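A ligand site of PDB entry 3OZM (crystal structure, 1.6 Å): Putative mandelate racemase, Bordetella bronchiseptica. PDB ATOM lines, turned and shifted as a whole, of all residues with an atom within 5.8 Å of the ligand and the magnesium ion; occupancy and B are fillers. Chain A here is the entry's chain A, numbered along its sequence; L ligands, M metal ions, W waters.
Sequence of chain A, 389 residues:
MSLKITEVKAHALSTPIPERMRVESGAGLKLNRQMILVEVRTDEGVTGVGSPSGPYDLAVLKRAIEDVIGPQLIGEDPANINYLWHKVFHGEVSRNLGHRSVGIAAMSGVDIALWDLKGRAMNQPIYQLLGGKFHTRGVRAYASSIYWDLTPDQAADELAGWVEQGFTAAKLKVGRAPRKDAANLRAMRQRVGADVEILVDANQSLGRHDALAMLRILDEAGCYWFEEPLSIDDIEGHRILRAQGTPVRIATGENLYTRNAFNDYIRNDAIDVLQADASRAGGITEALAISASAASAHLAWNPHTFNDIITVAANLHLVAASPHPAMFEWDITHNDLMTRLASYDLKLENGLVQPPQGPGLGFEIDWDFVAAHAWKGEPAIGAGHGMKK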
ATOM      1  N   SER A  25     -35.647 -24.872 -18.293  1.00  0.00           N
ATOM      2  CA  SER A  25     -34.343 -24.997 -17.673  1.00  0.00           C
ATOM      3  C   SER A  25     -34.493 -24.577 -16.212  1.00  0.00           C
ATOM      4  O   SER A  25     -35.608 -24.399 -15.726  1.00  0.00           O
ATOM      5  CB  SER A  25     -33.339 -24.068 -18.348  1.00  0.00           C
ATOM      6  OG  SER A  25     -33.730 -22.724 -18.155  1.00  0.00           O
ATOM      7  N   GLY A  26     -33.364 -24.420 -15.516  1.00  0.00           N
ATOM      8  CA  GLY A  26     -33.396 -23.940 -14.150  1.00  0.00           C
ATOM      9  C   GLY A  26     -34.118 -22.610 -14.012  1.00  0.00           C
ATOM     10  O   GLY A  26     -34.608 -22.275 -12.934  1.00  0.00           O
ATOM     11  N   ALA A  27     -34.180 -21.849 -15.108  1.00  0.00           N
ATOM     12  CA  ALA A  27     -34.828 -20.536 -15.119  1.00  0.00           C
ATOM     13  C   ALA A  27     -36.363 -20.620 -15.164  1.00  0.00           C
ATOM     14  O   ALA A  27     -37.051 -19.625 -14.923  1.00  0.00           O
ATOM     15  CB  ALA A  27     -34.306 -19.685 -16.294  1.00  0.00           C
ATOM     16  N   LYS A  30     -40.620 -21.852 -20.291  1.00  0.00           N
ATOM     17  CA  LYS A  30     -41.002 -20.710 -21.125  1.00  0.00           C
ATOM     18  C   LYS A  30     -42.447 -20.835 -21.598  1.00  0.00           C
ATOM     19  O   LYS A  30     -42.898 -21.913 -22.006  1.00  0.00           O
ATOM     20  CB  LYS A  30     -40.053 -20.566 -22.323  1.00  0.00           C
ATOM     21  CG  LYS A  30     -38.562 -20.418 -21.920  1.00  0.00           C
ATOM     22  CD  LYS A  30     -37.668 -20.066 -23.118  1.00  0.00           C
ATOM     23  CE  LYS A  30     -36.203 -20.241 -22.738  1.00  0.00           C
ATOM     24  NZ  LYS A  30     -35.893 -19.392 -21.554  1.00  0.00           N
ATOM     25  N   GLY A  54     -34.973  -9.898 -20.591  1.00  0.00           N
ATOM     26  CA  GLY A  54     -36.045 -10.564 -19.873  1.00  0.00           C
ATOM     27  C   GLY A  54     -35.575 -11.964 -19.509  1.00  0.00           C
ATOM     28  O   GLY A  54     -34.470 -12.362 -19.863  1.00  0.00           O
ATOM     29  N   PRO A  55     -36.415 -12.735 -18.806  1.00  0.00           N
ATOM     30  CA  PRO A  55     -37.747 -12.368 -18.323  1.00  0.00           C
ATOM     31  C   PRO A  55     -37.696 -11.470 -17.098  1.00  0.00           C
ATOM     32  O   PRO A  55     -37.047 -11.800 -16.080  1.00  0.00           O
ATOM     33  CB  PRO A  55     -38.363 -13.726 -17.973  1.00  0.00           C
ATOM     34  CG  PRO A  55     -37.193 -14.574 -17.611  1.00  0.00           C
ATOM     35  CD  PRO A  55     -36.108 -14.150 -18.563  1.00  0.00           C
ATOM     36  N   TYR A 142     -22.662 -19.746 -31.012  1.00  0.00           N
ATOM     37  CA  TYR A 142     -23.112 -21.041 -30.515  1.00  0.00           C
ATOM     38  C   TYR A 142     -24.634 -21.116 -30.467  1.00  0.00           C
ATOM     39  O   TYR A 142     -25.317 -20.109 -30.237  1.00  0.00           O
ATOM     40  CB  TYR A 142     -22.453 -21.401 -29.170  1.00  0.00           C
ATOM     41  CG  TYR A 142     -22.953 -20.684 -27.920  1.00  0.00           C
ATOM     42  CD1 TYR A 142     -24.082 -21.138 -27.233  1.00  0.00           C
ATOM     43  CD2 TYR A 142     -22.257 -19.583 -27.400  1.00  0.00           C
ATOM     44  CE1 TYR A 142     -24.516 -20.508 -26.061  1.00  0.00           C
ATOM     45  CE2 TYR A 142     -22.676 -18.950 -26.244  1.00  0.00           C
ATOM     46  CZ  TYR A 142     -23.799 -19.412 -25.572  1.00  0.00           C
ATOM     47  OH  TYR A 142     -24.213 -18.789 -24.408  1.00  0.00           O
ATOM     48  N   SER A 144     -27.951 -21.858 -28.803  1.00  0.00           N
ATOM     49  CA  SER A 144     -28.446 -21.823 -27.431  1.00  0.00           C
ATOM     50  C   SER A 144     -29.945 -22.105 -27.413  1.00  0.00           C
ATOM     51  O   SER A 144     -30.724 -21.319 -27.955  1.00  0.00           O
ATOM     52  CB  SER A 144     -28.188 -20.423 -26.871  1.00  0.00           C
ATOM     53  OG  SER A 144     -28.457 -20.344 -25.485  1.00  0.00           O
ATOM     54  N   SER A 145     -30.388 -23.210 -26.813  1.00  0.00           N
ATOM     55  CA  SER A 145     -29.578 -24.254 -26.211  1.00  0.00           C
ATOM     56  C   SER A 145     -30.381 -25.528 -26.383  1.00  0.00           C
ATOM     57  O   SER A 145     -31.523 -25.491 -26.860  1.00  0.00           O
ATOM     58  CB  SER A 145     -29.407 -24.041 -24.703  1.00  0.00           C
ATOM     59  OG  SER A 145     -28.568 -22.944 -24.402  1.00  0.00           O
ATOM     60  N   TYR A 147     -32.320 -28.135 -24.197  1.00  0.00           N
ATOM     61  CA  TYR A 147     -32.930 -27.939 -22.882  1.00  0.00           C
ATOM     62  C   TYR A 147     -33.177 -29.235 -22.108  1.00  0.00           C
ATOM     63  O   TYR A 147     -32.796 -30.314 -22.561  1.00  0.00           O
ATOM     64  CB  TYR A 147     -34.222 -27.108 -23.004  1.00  0.00           C
ATOM     65  CG  TYR A 147     -33.933 -25.626 -23.074  1.00  0.00           C
ATOM     66  CD1 TYR A 147     -33.415 -25.051 -24.231  1.00  0.00           C
ATOM     67  CD2 TYR A 147     -34.157 -24.811 -21.976  1.00  0.00           C
ATOM     68  CE1 TYR A 147     -33.126 -23.692 -24.281  1.00  0.00           C
ATOM     69  CE2 TYR A 147     -33.890 -23.453 -22.028  1.00  0.00           C
ATOM     70  CZ  TYR A 147     -33.381 -22.899 -23.184  1.00  0.00           C
ATOM     71  OH  TYR A 147     -33.097 -21.552 -23.223  1.00  0.00           O
ATOM     72  N   LYS A 171     -24.899 -25.240 -26.620  1.00  0.00           N
ATOM     73  CA  LYS A 171     -24.998 -25.271 -25.161  1.00  0.00           C
ATOM     74  C   LYS A 171     -26.105 -26.213 -24.673  1.00  0.00           C
ATOM     75  O   LYS A 171     -27.189 -26.268 -25.280  1.00  0.00           O
ATOM     76  CB  LYS A 171     -25.244 -23.851 -24.618  1.00  0.00           C
ATOM     77  CG  LYS A 171     -25.163 -23.756 -23.098  1.00  0.00           C
ATOM     78  CD  LYS A 171     -24.888 -22.317 -22.595  1.00  0.00           C
ATOM     79  CE  LYS A 171     -26.159 -21.425 -22.644  1.00  0.00           C
ATOM     80  NZ  LYS A 171     -25.808 -19.999 -22.312  1.00  0.00           N
ATOM     81  N   LYS A 173     -28.481 -27.367 -21.360  1.00  0.00           N
ATOM     82  CA  LYS A 173     -29.006 -27.064 -20.045  1.00  0.00           C
ATOM     83  C   LYS A 173     -28.952 -28.287 -19.134  1.00  0.00           C
ATOM     84  O   LYS A 173     -29.292 -29.409 -19.546  1.00  0.00           O
ATOM     85  CB  LYS A 173     -30.450 -26.539 -20.150  1.00  0.00           C
ATOM     86  CG  LYS A 173     -30.569 -25.332 -21.037  1.00  0.00           C
ATOM     87  CD  LYS A 173     -29.876 -24.134 -20.410  1.00  0.00           C
ATOM     88  CE  LYS A 173     -30.119 -22.892 -21.245  1.00  0.00           C
ATOM     89  NZ  LYS A 173     -29.843 -21.661 -20.462  1.00  0.00           N
ATOM     90  N   ASP A 201     -24.841 -25.334 -19.038  1.00  0.00           N
ATOM     91  CA  ASP A 201     -25.456 -24.237 -18.287  1.00  0.00           C
ATOM     92  C   ASP A 201     -26.400 -24.823 -17.266  1.00  0.00           C
ATOM     93  O   ASP A 201     -27.408 -25.440 -17.614  1.00  0.00           O
ATOM     94  CB  ASP A 201     -26.226 -23.326 -19.252  1.00  0.00           C
ATOM     95  CG  ASP A 201     -26.782 -22.074 -18.583  1.00  0.00           C
ATOM     96  OD1 ASP A 201     -26.782 -21.960 -17.331  1.00  0.00           O
ATOM     97  OD2 ASP A 201     -27.221 -21.198 -19.336  1.00  0.00           O
ATOM     98  N   ASN A 203     -27.962 -22.954 -14.814  1.00  0.00           N
ATOM     99  CA  ASN A 203     -28.915 -21.980 -14.310  1.00  0.00           C
ATOM    100  C   ASN A 203     -29.016 -21.929 -12.777  1.00  0.00           C
ATOM    101  O   ASN A 203     -30.114 -21.879 -12.224  1.00  0.00           O
ATOM    102  CB  ASN A 203     -30.305 -22.237 -14.904  1.00  0.00           C
ATOM    103  CG  ASN A 203     -30.355 -21.891 -16.380  1.00  0.00           C
ATOM    104  OD1 ASN A 203     -30.206 -22.762 -17.240  1.00  0.00           O
ATOM    105  ND2 ASN A 203     -30.560 -20.614 -16.678  1.00  0.00           N
ATOM    106  N   GLU A 227     -21.483 -22.908 -17.084  1.00  0.00           N
ATOM    107  CA  GLU A 227     -22.167 -21.628 -16.859  1.00  0.00           C
ATOM    108  C   GLU A 227     -23.164 -21.708 -15.711  1.00  0.00           C
ATOM    109  O   GLU A 227     -23.891 -22.683 -15.569  1.00  0.00           O
ATOM    110  CB  GLU A 227     -22.896 -21.228 -18.151  1.00  0.00           C
ATOM    111  CG  GLU A 227     -23.867 -20.057 -18.008  1.00  0.00           C
ATOM    112  CD  GLU A 227     -24.361 -19.573 -19.362  1.00  0.00           C
ATOM    113  OE1 GLU A 227     -23.838 -20.002 -20.408  1.00  0.00           O
ATOM    114  OE2 GLU A 227     -25.286 -18.734 -19.367  1.00  0.00           O
ATOM    115  N   GLU A 228     -23.202 -20.642 -14.898  1.00  0.00           N
ATOM    116  CA  GLU A 228     -23.988 -20.598 -13.669  1.00  0.00           C
ATOM    117  C   GLU A 228     -24.082 -21.957 -12.962  1.00  0.00           C
ATOM    118  O   GLU A 228     -25.178 -22.490 -12.749  1.00  0.00           O
ATOM    119  CB  GLU A 228     -25.397 -20.031 -13.923  1.00  0.00           C
ATOM    120  CG  GLU A 228     -25.464 -18.526 -14.272  1.00  0.00           C
ATOM    121  CD  GLU A 228     -26.904 -17.978 -14.160  1.00  0.00           C
ATOM    122  OE1 GLU A 228     -27.840 -18.680 -14.599  1.00  0.00           O
ATOM    123  OE2 GLU A 228     -27.097 -16.857 -13.626  1.00  0.00           O
ATOM    124  N   GLU A 254     -25.128 -13.578 -16.467  1.00  0.00           N
ATOM    125  CA  GLU A 254     -26.435 -13.112 -16.911  1.00  0.00           C
ATOM    126  C   GLU A 254     -27.281 -12.545 -15.767  1.00  0.00           C
ATOM    127  O   GLU A 254     -28.179 -11.736 -15.992  1.00  0.00           O
ATOM    128  CB  GLU A 254     -27.187 -14.220 -17.636  1.00  0.00           C
ATOM    129  CG  GLU A 254     -27.841 -15.216 -16.738  1.00  0.00           C
ATOM    130  CD  GLU A 254     -28.292 -16.428 -17.526  1.00  0.00           C
ATOM    131  OE1 GLU A 254     -29.471 -16.816 -17.461  1.00  0.00           O
ATOM    132  OE2 GLU A 254     -27.451 -16.971 -18.223  1.00  0.00           O
ATOM    133  N   GLN A 275     -20.011 -13.011 -18.290  1.00  0.00           N
ATOM    134  CA  GLN A 275     -21.120 -13.063 -19.243  1.00  0.00           C
ATOM    135  C   GLN A 275     -22.068 -11.861 -19.170  1.00  0.00           C
ATOM    136  O   GLN A 275     -23.212 -11.951 -19.606  1.00  0.00           O
ATOM    137  CB  GLN A 275     -21.889 -14.386 -19.088  1.00  0.00           C
ATOM    138  CG  GLN A 275     -20.988 -15.600 -19.402  1.00  0.00           C
ATOM    139  CD  GLN A 275     -21.745 -16.922 -19.327  1.00  0.00           C
ATOM    140  OE1 GLN A 275     -22.249 -17.301 -18.273  1.00  0.00           O
ATOM    141  NE2 GLN A 275     -21.808 -17.632 -20.442  1.00  0.00           N
ATOM    142  N   ARG A 280     -28.657  -6.157 -19.831  1.00  0.00           N
ATOM    143  CA  ARG A 280     -29.043  -6.479 -18.451  1.00  0.00           C
ATOM    144  C   ARG A 280     -28.150  -5.804 -17.427  1.00  0.00           C
ATOM    145  O   ARG A 280     -28.629  -5.265 -16.430  1.00  0.00           O
ATOM    146  CB  ARG A 280     -29.018  -8.002 -18.217  1.00  0.00           C
ATOM    147  CG  ARG A 280     -29.964  -8.780 -19.102  1.00  0.00           C
ATOM    148  CD  ARG A 280     -29.691 -10.283 -19.060  1.00  0.00           C
ATOM    149  NE  ARG A 280     -30.073 -10.914 -17.789  1.00  0.00           N
ATOM    150  CZ  ARG A 280     -31.304 -11.350 -17.535  1.00  0.00           C
ATOM    151  NH1 ARG A 280     -32.268 -11.216 -18.450  1.00  0.00           N
ATOM    152  NH2 ARG A 280     -31.582 -11.940 -16.376  1.00  0.00           N
ATOM    153  N   HIS A 304     -23.920 -13.087 -22.238  1.00  0.00           N
ATOM    154  CA  HIS A 304     -25.273 -13.601 -22.387  1.00  0.00           C
ATOM    155  C   HIS A 304     -26.006 -12.647 -23.352  1.00  0.00           C
ATOM    156  O   HIS A 304     -25.789 -11.418 -23.290  1.00  0.00           O
ATOM    157  CB  HIS A 304     -25.945 -13.617 -21.015  1.00  0.00           C
ATOM    158  CG  HIS A 304     -27.415 -13.932 -21.044  1.00  0.00           C
ATOM    159  ND1 HIS A 304     -28.383 -12.971 -21.237  1.00  0.00           N
ATOM    160  CD2 HIS A 304     -28.073 -15.109 -20.864  1.00  0.00           C
ATOM    161  CE1 HIS A 304     -29.578 -13.540 -21.183  1.00  0.00           C
ATOM    162  NE2 HIS A 304     -29.416 -14.833 -20.947  1.00  0.00           N
ATOM    163  N   THR A 305     -26.839 -13.185 -24.235  1.00  0.00           N
ATOM    164  CA  THR A 305     -27.520 -12.353 -25.243  1.00  0.00           C
ATOM    165  C   THR A 305     -29.013 -12.694 -25.395  1.00  0.00           C
ATOM    166  O   THR A 305     -29.708 -12.098 -26.227  1.00  0.00           O
ATOM    167  CB  THR A 305     -26.908 -12.540 -26.633  1.00  0.00           C
ATOM    168  OG1 THR A 305     -27.274 -13.830 -27.161  1.00  0.00           O
ATOM    169  CG2 THR A 305     -25.392 -12.382 -26.617  1.00  0.00           C
ATOM    170  N   PHE A 306     -29.501 -13.608 -24.574  1.00  0.00           N
ATOM    171  CA  PHE A 306     -30.764 -14.329 -24.801  1.00  0.00           C
ATOM    172  C   PHE A 306     -32.029 -13.555 -24.390  1.00  0.00           C
ATOM    173  O   PHE A 306     -32.318 -13.392 -23.203  1.00  0.00           O
ATOM    174  CB  PHE A 306     -30.663 -15.653 -24.026  1.00  0.00           C
ATOM    175  CG  PHE A 306     -31.632 -16.735 -24.437  1.00  0.00           C
ATOM    176  CD1 PHE A 306     -31.238 -17.749 -25.320  1.00  0.00           C
ATOM    177  CD2 PHE A 306     -32.895 -16.808 -23.876  1.00  0.00           C
ATOM    178  CE1 PHE A 306     -32.100 -18.782 -25.660  1.00  0.00           C
ATOM    179  CE2 PHE A 306     -33.778 -17.843 -24.218  1.00  0.00           C
ATOM    180  CZ  PHE A 306     -33.377 -18.826 -25.100  1.00  0.00           C
ATOM    181  N   GLU A 329     -23.566 -16.172 -28.127  1.00  0.00           N
ATOM    182  CA  GLU A 329     -24.827 -16.871 -27.888  1.00  0.00           C
ATOM    183  C   GLU A 329     -25.882 -16.496 -28.915  1.00  0.00           C
ATOM    184  O   GLU A 329     -26.198 -15.313 -29.081  1.00  0.00           O
ATOM    185  CB  GLU A 329     -25.361 -16.560 -26.483  1.00  0.00           C
ATOM    186  CG  GLU A 329     -26.645 -17.322 -26.155  1.00  0.00           C
ATOM    187  CD  GLU A 329     -27.084 -17.190 -24.719  1.00  0.00           C
ATOM    188  OE1 GLU A 329     -26.810 -16.152 -24.084  1.00  0.00           O
ATOM    189  OE2 GLU A 329     -27.748 -18.144 -24.233  1.00  0.00           O
ATOM    190  N   ILE A 381     -42.864 -16.800 -18.198  1.00  0.00           N
ATOM    191  CA  ILE A 381     -42.128 -17.987 -17.776  1.00  0.00           C
ATOM    192  C   ILE A 381     -42.689 -18.524 -16.468  1.00  0.00           C
ATOM    193  O   ILE A 381     -43.156 -17.753 -15.625  1.00  0.00           O
ATOM    194  CB  ILE A 381     -40.620 -17.669 -17.676  1.00  0.00           C
ATOM    195  CG1 ILE A 381     -39.774 -18.949 -17.587  1.00  0.00           C
ATOM    196  CG2 ILE A 381     -40.316 -16.714 -16.532  1.00  0.00           C
ATOM    197  CD1 ILE A 381     -38.290 -18.687 -17.849  1.00  0.00           C
HETATM  198  O1  LIG L   1     -33.385 -20.233 -21.035  1.00  0.00           O
HETATM  199  O2  LIG L   1     -33.731 -17.757 -19.957  1.00  0.00           O
HETATM  200  O3  LIG L   1     -29.678 -19.081 -19.055  1.00  0.00           O
HETATM  201  O4  LIG L   1     -29.404 -17.970 -22.479  1.00  0.00           O
HETATM  202  O5  LIG L   1     -32.228 -20.821 -19.239  1.00  0.00           O
HETATM  203  C1  LIG L   1     -32.746 -19.969 -20.007  1.00  0.00           C
HETATM  204  C2  LIG L   1     -32.545 -18.498 -19.633  1.00  0.00           C
HETATM  205  C3  LIG L   1     -31.370 -17.914 -20.443  1.00  0.00           C
HETATM  206  C4  LIG L   1     -30.147 -18.851 -20.391  1.00  0.00           C
HETATM  207  C5  LIG L   1     -29.033 -18.449 -21.389  1.00  0.00           C
HETATM  208  O6  LIG L   1     -27.826 -18.643 -21.072  1.00  0.00           O
HETATM  209  O7  LIG L   1     -31.095 -16.592 -19.974  1.00  0.00           O
HETATM  210 MG    MG M   1     -27.436 -19.024 -18.912  1.00  0.00          MG
HETATM  211  O   HOH W   1     -30.378 -20.798 -23.540  1.00  0.00           O
HETATM  212  O   HOH W   2     -36.010 -21.288 -19.339  1.00  0.00           O
HETATM  213  O   HOH W   3     -33.613 -14.597 -20.911  1.00  0.00           O
HETATM  214  O   HOH W   4     -27.417 -19.445 -16.860  1.00  0.00           O
HETATM  215  O   HOH W   5     -25.118 -16.961 -21.539  1.00  0.00           O
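NE of Arg 280 lies within hydrogen-bond range of O of Glu 254 (2.7 Å). OE1 of Glu 227 is in salt-bridge range of NZ of Lys 171, at 2.7 Å. OE1 of Glu 227 lies within hydrogen-bond range of NE2 of Gln 275 (3.1 Å). The side-chain carboxylate (OD2) of Asp 201 lies close to the side-chain amino group (NZ) of Lys 173 (2.9 Å). The side-chain carboxylate (OD1) of Asp 201 lies within hydrogen-bond range of the backbone NH (N) of Asn 203. The side-chain hydroxyl (OG1) of Thr 305 sits at hydrogen-bond distance from the backbone carbonyl oxygen (O) of Glu 329. The side-chain amino group (NZ) of Lys 171 sits at hydrogen-bond distance from the side-chain hydroxyl (OH) of Tyr 142, at 2.9 Å. The side-chain hydroxyl of Ser 144 is in hydrogen-bond range of the side-chain hydroxyl of Ser 145 (2.8 Å).
The magnesium ion is bound by water W4, the side-chain carboxylate (OE2) of Glu 254, the side-chain carboxylate (OE2) of Glu 227, the side-chain carboxylate (OD2) of Asp 201, an oxygen (O6) of the ligand and an oxygen (O3) of the ligand.
Residues that only touch the magnesium ion: Lys 173 and Lys 171. Of the 24 residues printed, 5 come within 4 Å of the magnesium ion.
Water W1 lies within hydrogen-bond range of OG of Ser 144, OH of Tyr 147, OG of Ser 145, O4 of the ligand and NZ of Lys 173. Water W5 lies within hydrogen-bond range of the side-chain carboxylate of Glu 329 (3.2 Å), the side-chain amino group of Lys 171 (3.2 Å) and the side-chain carboxylate of Glu 227 (3.5 Å). Water W2 lies within hydrogen-bond range of the side-chain amino group of Lys 30, the side-chain hydroxyl of Ser 25 and an oxygen (O1) of the ligand. Water W3 lies within hydrogen-bond range of the backbone carbonyl oxygen of Gly 54 (2.6 Å), the backbone carbonyl oxygen of Phe 306 (2.9 Å) and an oxygen (O2) of the ligand (3.3 Å).
Residues that only touch the ligand: Ala 27, Ser 144 and Phe 306. Of the 24 residues printed, 14 come within 4 Å of the ligand.
O4 of the ligand sits close to OE2 of Glu 329, 2.4 Å away. An oxygen (O1) of the ligand sits at hydrogen-bond distance from the side-chain hydroxyl (OH) of Tyr 147. NE2 of His 304 is in hydrogen-bond range of O7 of the ligand (2.6 Å). The side-chain hydroxyl (OG) of Ser 25 lies within hydrogen-bond range of an oxygen (O5) of the ligand (2.7 Å). The side-chain amino group of Lys 30 lies within salt-bridge range of an oxygen (O1) of the ligand, 2.7 Å away. An oxygen (O6) of the ligand sits close to the side-chain amino group (NZ) of Lys 171 (2.7 Å). The side-chain amino group (NZ) of Lys 173 is in salt-bridge range of an oxygen (O5) of the ligand, at 2.8 Å. O5 of the ligand lies within hydrogen-bond range of ND2 of Asn 203.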
